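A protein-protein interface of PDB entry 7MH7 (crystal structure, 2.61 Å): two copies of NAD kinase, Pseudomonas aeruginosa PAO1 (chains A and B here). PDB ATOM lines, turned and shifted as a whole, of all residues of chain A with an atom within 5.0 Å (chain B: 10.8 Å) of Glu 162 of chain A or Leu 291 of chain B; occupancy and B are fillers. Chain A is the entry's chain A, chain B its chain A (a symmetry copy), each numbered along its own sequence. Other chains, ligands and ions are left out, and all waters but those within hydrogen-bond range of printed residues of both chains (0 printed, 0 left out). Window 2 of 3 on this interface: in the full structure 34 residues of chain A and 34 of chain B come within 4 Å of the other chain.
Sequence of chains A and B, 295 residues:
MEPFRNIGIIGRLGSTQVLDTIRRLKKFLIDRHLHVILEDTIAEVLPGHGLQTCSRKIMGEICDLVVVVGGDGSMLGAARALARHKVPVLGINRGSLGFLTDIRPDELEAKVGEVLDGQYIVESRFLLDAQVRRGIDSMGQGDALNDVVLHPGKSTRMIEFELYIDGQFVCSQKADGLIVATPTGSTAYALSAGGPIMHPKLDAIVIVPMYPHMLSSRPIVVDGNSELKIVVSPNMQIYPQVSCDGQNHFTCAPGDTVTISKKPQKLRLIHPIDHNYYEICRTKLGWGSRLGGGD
No position is printed for both chains.
Of the 8 pairs that touch across the chains among the printed residues, none has its exchanged pair printed and touching as well.
The side-chain carboxylate of Glu 162 of chain A is in hydrogen-bond range of the side-chain hydroxyl of Tyr 164 of chain A, at 3.2 Å.
O of Val 231 of chain A lies within hydrogen-bond range of N of Glu 162 of chain A (2.9 Å).
The backbone carbonyl oxygen (O) of Arg 282 of chain B sits at hydrogen-bond distance from the backbone NH (N) of Trp 287 of chain B (3.2 Å).
The backbone NH (N) of Leu 163 of chain A lies within hydrogen-bond range of the backbone carbonyl oxygen (O) of Cys 171 of chain A, 3.0 Å away.
Phe 169 of chain A touches Ser 289 of chain B.
Phe 169 of chain A touches Arg 290 of chain B (CZ to N, 3.7 Å).
CB of Trp 287 of chain B touches CB of Cys 171 of chain A (3.8 Å).
Cys 171 of chain A touches Gly 288 of chain B.
Glu 162 of chain A touches just one residue of chain B: Leu 291.
Printed residues of chain A within 4 Å of Leu 291 of chain B: Glu 162.
No residue of chain B comes within 4 Å of Leu 163 of chain A.
Of chain B, only Gly 288 and Ser 289 come within 4 Å of Ser 172 of chain A.
No residue of chain B comes within 4 Å of Ile 230 of chain A.
No residue of chain B comes within 4 Å of Val 231 of chain A.
Ser 233 of chain A touches none of the printed residues of chain B.
Of the printed residues of chain A, Arg 282 of chain B touches Phe 169.
Of the printed residues of chain A, Trp 287 of chain B touches Cys 171.
Of the printed residues of chain A, Gly 288 of chain B touches Cys 171 (3.5 Å) and Ser 172 (3.2 Å).
Printed residues of chain B within 4 Å of Cys 171 of chain A: Trp 287 (3.8 Å) and Gly 288 (3.5 Å).
Of the printed residues of chain A, Ser 289 of chain B touches Phe 169 and Ser 172.
The nearest residue of chain B that does not touch Glu 162 of chain A is Arg 290 of chain B (4.1 Å).
Of the 6 printed residues of chain B, 6 touch a printed residue of chain A.
Hydrophobic or aromatic side chains of chain B that line the printed part of chain A: Trp 287 and Leu 291.
Of the 13 printed residues of chain A, 4 touch a printed residue of chain B.
Hydrophobic or aromatic side chains of chain A within 4 Å of the printed part of chain B: Phe 169.
O of Ser 289 of chain B is in hydrogen-bond range of OG of Ser 172 of chain A, 2.5 Å away.
The side-chain carboxylate (OE2) of Glu 162 of chain A lies within hydrogen-bond range of the backbone NH (N) of Leu 291 of chain B (3.1 Å).
The guanidinium group of Arg 282 of chain B sits at hydrogen-bond distance from the backbone carbonyl oxygen of Phe 169 of chain A.
N of Ser 172 of chain A is in hydrogen-bond range of O of Gly 288 of chain B.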
ATOM      1  N   GLU A 160      15.279   6.386  13.604  1.00  0.00           N
ATOM      2  CA  GLU A 160      15.597   6.589  12.198  1.00  0.00           C
ATOM      3  C   GLU A 160      14.728   7.710  11.652  1.00  0.00           C
ATOM      4  O   GLU A 160      13.552   7.826  12.011  1.00  0.00           O
ATOM      5  CB  GLU A 160      15.386   5.303  11.391  1.00  0.00           C
ATOM      6  CG  GLU A 160      16.189   4.117  11.902  1.00  0.00           C
ATOM      7  CD  GLU A 160      15.909   2.845  11.129  1.00  0.00           C
ATOM      8  OE1 GLU A 160      15.264   2.927  10.063  1.00  0.00           O
ATOM      9  OE2 GLU A 160      16.331   1.763  11.588  1.00  0.00           O
ATOM     10  N   PHE A 161      15.307   8.536  10.785  1.00  0.00           N
ATOM     11  CA  PHE A 161      14.607   9.710  10.287  1.00  0.00           C
ATOM     12  C   PHE A 161      15.287  10.202   9.018  1.00  0.00           C
ATOM     13  O   PHE A 161      16.399   9.792   8.681  1.00  0.00           O
ATOM     14  CB  PHE A 161      14.563  10.820  11.343  1.00  0.00           C
ATOM     15  CG  PHE A 161      15.912  11.181  11.901  1.00  0.00           C
ATOM     16  CD1 PHE A 161      16.691  12.155  11.297  1.00  0.00           C
ATOM     17  CD2 PHE A 161      16.403  10.543  13.029  1.00  0.00           C
ATOM     18  CE1 PHE A 161      17.933  12.485  11.807  1.00  0.00           C
ATOM     19  CE2 PHE A 161      17.643  10.869  13.544  1.00  0.00           C
ATOM     20  CZ  PHE A 161      18.409  11.842  12.933  1.00  0.00           C
ATOM     21  N   GLU A 162      14.593  11.096   8.318  1.00  0.00           N
ATOM     22  CA  GLU A 162      15.123  11.793   7.158  1.00  0.00           C
ATOM     23  C   GLU A 162      15.171  13.287   7.447  1.00  0.00           C
ATOM     24  O   GLU A 162      14.314  13.824   8.156  1.00  0.00           O
ATOM     25  CB  GLU A 162      14.269  11.540   5.909  1.00  0.00           C
ATOM     26  CG  GLU A 162      14.239  10.099   5.431  1.00  0.00           C
ATOM     27  CD  GLU A 162      13.249   9.892   4.300  1.00  0.00           C
ATOM     28  OE1 GLU A 162      12.243  10.632   4.248  1.00  0.00           O
ATOM     29  OE2 GLU A 162      13.475   8.996   3.461  1.00  0.00           O
ATOM     30  N   LEU A 163      16.173  13.957   6.888  1.00  0.00           N
ATOM     31  CA  LEU A 163      16.349  15.392   7.058  1.00  0.00           C
ATOM     32  C   LEU A 163      16.103  16.099   5.732  1.00  0.00           C
ATOM     33  O   LEU A 163      16.612  15.669   4.691  1.00  0.00           O
ATOM     34  CB  LEU A 163      17.751  15.718   7.579  1.00  0.00           C
ATOM     35  CG  LEU A 163      18.073  17.204   7.764  1.00  0.00           C
ATOM     36  CD1 LEU A 163      17.078  17.851   8.717  1.00  0.00           C
ATOM     37  CD2 LEU A 163      19.500  17.394   8.259  1.00  0.00           C
ATOM     38  N   TYR A 164      15.322  17.176   5.774  1.00  0.00           N
ATOM     39  CA  TYR A 164      15.046  18.000   4.606  1.00  0.00           C
ATOM     40  C   TYR A 164      15.314  19.456   4.954  1.00  0.00           C
ATOM     41  O   TYR A 164      14.839  19.948   5.983  1.00  0.00           O
ATOM     42  CB  TYR A 164      13.599  17.831   4.126  1.00  0.00           C
ATOM     43  CG  TYR A 164      13.289  16.475   3.532  1.00  0.00           C
ATOM     44  CD1 TYR A 164      12.862  15.425   4.333  1.00  0.00           C
ATOM     45  CD2 TYR A 164      13.413  16.248   2.168  1.00  0.00           C
ATOM     46  CE1 TYR A 164      12.574  14.186   3.794  1.00  0.00           C
ATOM     47  CE2 TYR A 164      13.126  15.012   1.619  1.00  0.00           C
ATOM     48  CZ  TYR A 164      12.707  13.985   2.437  1.00  0.00           C
ATOM     49  OH  TYR A 164      12.421  12.753   1.896  1.00  0.00           O
ATOM     50  N   PHE A 169      16.309  17.067  -0.077  1.00  0.00           N
ATOM     51  CA  PHE A 169      16.677  15.911   0.730  1.00  0.00           C
ATOM     52  C   PHE A 169      18.165  15.936   1.058  1.00  0.00           C
ATOM     53  O   PHE A 169      19.008  16.085   0.168  1.00  0.00           O
ATOM     54  CB  PHE A 169      16.313  14.617   0.003  1.00  0.00           C
ATOM     55  CG  PHE A 169      16.790  13.373   0.700  1.00  0.00           C
ATOM     56  CD1 PHE A 169      16.173  12.927   1.858  1.00  0.00           C
ATOM     57  CD2 PHE A 169      17.853  12.646   0.190  1.00  0.00           C
ATOM     58  CE1 PHE A 169      16.613  11.782   2.498  1.00  0.00           C
ATOM     59  CE2 PHE A 169      18.297  11.500   0.826  1.00  0.00           C
ATOM     60  CZ  PHE A 169      17.675  11.067   1.979  1.00  0.00           C
ATOM     61  N   CYS A 171      19.760  13.611   3.884  1.00  0.00           N
ATOM     62  CA  CYS A 171      20.164  12.232   4.138  1.00  0.00           C
ATOM     63  C   CYS A 171      19.136  11.568   5.043  1.00  0.00           C
ATOM     64  O   CYS A 171      18.323  12.234   5.689  1.00  0.00           O
ATOM     65  CB  CYS A 171      21.558  12.162   4.773  1.00  0.00           C
ATOM     66  SG  CYS A 171      21.663  12.865   6.439  1.00  0.00           S
ATOM     67  N   SER A 172      19.174  10.238   5.063  1.00  0.00           N
ATOM     68  CA  SER A 172      18.536   9.439   6.098  1.00  0.00           C
ATOM     69  C   SER A 172      19.603   8.983   7.084  1.00  0.00           C
ATOM     70  O   SER A 172      20.774   8.831   6.725  1.00  0.00           O
ATOM     71  CB  SER A 172      17.808   8.228   5.507  1.00  0.00           C
ATOM     72  OG  SER A 172      18.720   7.295   4.950  1.00  0.00           O
ATOM     73  N   LYS A 229      12.921  20.064   7.927  1.00  0.00           N
ATOM     74  CA  LYS A 229      11.810  19.116   7.915  1.00  0.00           C
ATOM     75  C   LYS A 229      12.362  17.745   8.278  1.00  0.00           C
ATOM     76  O   LYS A 229      13.083  17.133   7.482  1.00  0.00           O
ATOM     77  CB  LYS A 229      11.121  19.093   6.551  1.00  0.00           C
ATOM     78  CG  LYS A 229       9.629  18.813   6.608  1.00  0.00           C
ATOM     79  CD  LYS A 229       8.971  19.115   5.270  1.00  0.00           C
ATOM     80  CE  LYS A 229       9.177  20.570   4.870  1.00  0.00           C
ATOM     81  NZ  LYS A 229       8.653  20.860   3.505  1.00  0.00           N
ATOM     82  N   ILE A 230      12.036  17.270   9.476  1.00  0.00           N
ATOM     83  CA  ILE A 230      12.470  15.966   9.959  1.00  0.00           C
ATOM     84  C   ILE A 230      11.296  15.005   9.835  1.00  0.00           C
ATOM     85  O   ILE A 230      10.221  15.252  10.393  1.00  0.00           O
ATOM     86  CB  ILE A 230      12.971  16.040  11.409  1.00  0.00           C
ATOM     87  CG1 ILE A 230      14.140  17.020  11.522  1.00  0.00           C
ATOM     88  CG2 ILE A 230      13.376  14.660  11.903  1.00  0.00           C
ATOM     89  CD1 ILE A 230      14.633  17.220  12.938  1.00  0.00           C
ATOM     90  N   VAL A 231      11.497  13.912   9.107  1.00  0.00           N
ATOM     91  CA  VAL A 231      10.462  12.912   8.871  1.00  0.00           C
ATOM     92  C   VAL A 231      10.852  11.655   9.635  1.00  0.00           C
ATOM     93  O   VAL A 231      11.858  11.010   9.314  1.00  0.00           O
ATOM     94  CB  VAL A 231      10.282  12.617   7.376  1.00  0.00           C
ATOM     95  CG1 VAL A 231       9.105  11.679   7.159  1.00  0.00           C
ATOM     96  CG2 VAL A 231      10.097  13.910   6.599  1.00  0.00           C
ATOM     97  N   SER A 233      10.924   7.854  10.676  1.00  0.00           N
ATOM     98  CA  SER A 233      10.869   6.656   9.847  1.00  0.00           C
ATOM     99  C   SER A 233       9.494   6.003   9.932  1.00  0.00           C
ATOM    100  O   SER A 233       9.063   5.624  11.031  1.00  0.00           O
ATOM    101  CB  SER A 233      11.944   5.663  10.276  1.00  0.00           C
ATOM    102  OG  SER A 233      11.816   4.441   9.573  1.00  0.00           O
ATOM    103  N   PRO A 234       8.775   5.858   8.816  1.00  0.00           N
ATOM    104  CA  PRO A 234       7.470   5.184   8.881  1.00  0.00           C
ATOM    105  C   PRO A 234       7.586   3.682   9.064  1.00  0.00           C
ATOM    106  O   PRO A 234       6.678   3.066   9.634  1.00  0.00           O
ATOM    107  CB  PRO A 234       6.817   5.540   7.535  1.00  0.00           C
ATOM    108  CG  PRO A 234       7.677   6.634   6.939  1.00  0.00           C
ATOM    109  CD  PRO A 234       9.050   6.394   7.473  1.00  0.00           C
ATOM    110  N   ARG B 282      26.427  13.108   0.298  1.00  0.00           N
ATOM    111  CA  ARG B 282      26.039  11.708   0.453  1.00  0.00           C
ATOM    112  C   ARG B 282      27.048  10.765  -0.189  1.00  0.00           C
ATOM    113  O   ARG B 282      27.204   9.627   0.268  1.00  0.00           O
ATOM    114  CB  ARG B 282      24.650  11.476  -0.140  1.00  0.00           C
ATOM    115  CG  ARG B 282      23.512  12.000   0.718  1.00  0.00           C
ATOM    116  CD  ARG B 282      22.167  11.505   0.212  1.00  0.00           C
ATOM    117  NE  ARG B 282      21.847  12.030  -1.111  1.00  0.00           N
ATOM    118  CZ  ARG B 282      21.250  13.194  -1.328  1.00  0.00           C
ATOM    119  NH1 ARG B 282      20.906  13.990  -0.329  1.00  0.00           N
ATOM    120  NH2 ARG B 282      20.992  13.568  -2.578  1.00  0.00           N
ATOM    121  N   TRP B 287      26.794   9.239   3.444  1.00  0.00           N
ATOM    122  CA  TRP B 287      25.532   9.363   4.161  1.00  0.00           C
ATOM    123  C   TRP B 287      24.448   8.506   3.517  1.00  0.00           C
ATOM    124  O   TRP B 287      24.473   8.227   2.314  1.00  0.00           O
ATOM    125  CB  TRP B 287      25.084  10.825   4.203  1.00  0.00           C
ATOM    126  CG  TRP B 287      25.991  11.722   4.989  1.00  0.00           C
ATOM    127  CD1 TRP B 287      27.068  11.350   5.743  1.00  0.00           C
ATOM    128  CD2 TRP B 287      25.900  13.147   5.098  1.00  0.00           C
ATOM    129  NE1 TRP B 287      27.651  12.457   6.313  1.00  0.00           N
ATOM    130  CE2 TRP B 287      26.952  13.572   5.933  1.00  0.00           C
ATOM    131  CE3 TRP B 287      25.028  14.106   4.569  1.00  0.00           C
ATOM    132  CZ2 TRP B 287      27.156  14.912   6.251  1.00  0.00           C
ATOM    133  CZ3 TRP B 287      25.233  15.435   4.887  1.00  0.00           C
ATOM    134  CH2 TRP B 287      26.289  15.827   5.719  1.00  0.00           C
ATOM    135  N   GLY B 288      23.489   8.085   4.336  1.00  0.00           N
ATOM    136  CA  GLY B 288      22.430   7.222   3.847  1.00  0.00           C
ATOM    137  C   GLY B 288      21.537   7.942   2.852  1.00  0.00           C
ATOM    138  O   GLY B 288      21.275   9.140   2.969  1.00  0.00           O
ATOM    139  N   SER B 289      21.066   7.196   1.859  1.00  0.00           N
ATOM    140  CA  SER B 289      20.217   7.744   0.812  1.00  0.00           C
ATOM    141  C   SER B 289      18.761   7.716   1.280  1.00  0.00           C
ATOM    142  O   SER B 289      18.482   7.685   2.481  1.00  0.00           O
ATOM    143  CB  SER B 289      20.438   6.971  -0.492  1.00  0.00           C
ATOM    144  OG  SER B 289      20.161   5.593  -0.322  1.00  0.00           O
ATOM    145  N   ARG B 290      17.820   7.724   0.338  1.00  0.00           N
ATOM    146  CA  ARG B 290      16.408   7.765   0.685  1.00  0.00           C
ATOM    147  C   ARG B 290      15.981   6.473   1.369  1.00  0.00           C
ATOM    148  O   ARG B 290      16.411   5.378   0.997  1.00  0.00           O
ATOM    149  CB  ARG B 290      15.559   8.004  -0.564  1.00  0.00           C
ATOM    150  CG  ARG B 290      14.677   9.243  -0.496  1.00  0.00           C
ATOM    151  CD  ARG B 290      15.034  10.237  -1.593  1.00  0.00           C
ATOM    152  NE  ARG B 290      14.143  11.393  -1.595  1.00  0.00           N
ATOM    153  CZ  ARG B 290      14.239  12.413  -2.436  1.00  0.00           C
ATOM    154  NH1 ARG B 290      15.184  12.459  -3.362  1.00  0.00           N
ATOM    155  NH2 ARG B 290      13.367  13.413  -2.346  1.00  0.00           N
ATOM    156  N   LEU B 291      15.128   6.610   2.379  1.00  0.00           N
ATOM    157  CA  LEU B 291      14.635   5.469   3.139  1.00  0.00           C
ATOM    158  C   LEU B 291      13.708   4.597   2.299  1.00  0.00           C
ATOM    159  O   LEU B 291      12.711   5.074   1.752  1.00  0.00           O
ATOM    160  CB  LEU B 291      13.913   5.947   4.399  1.00  0.00           C
ATOM    161  CG  LEU B 291      14.628   5.706   5.730  1.00  0.00           C
ATOM    162  CD1 LEU B 291      13.951   6.490   6.837  1.00  0.00           C
ATOM    163  CD2 LEU B 291      14.647   4.225   6.065  1.00  0.00           C
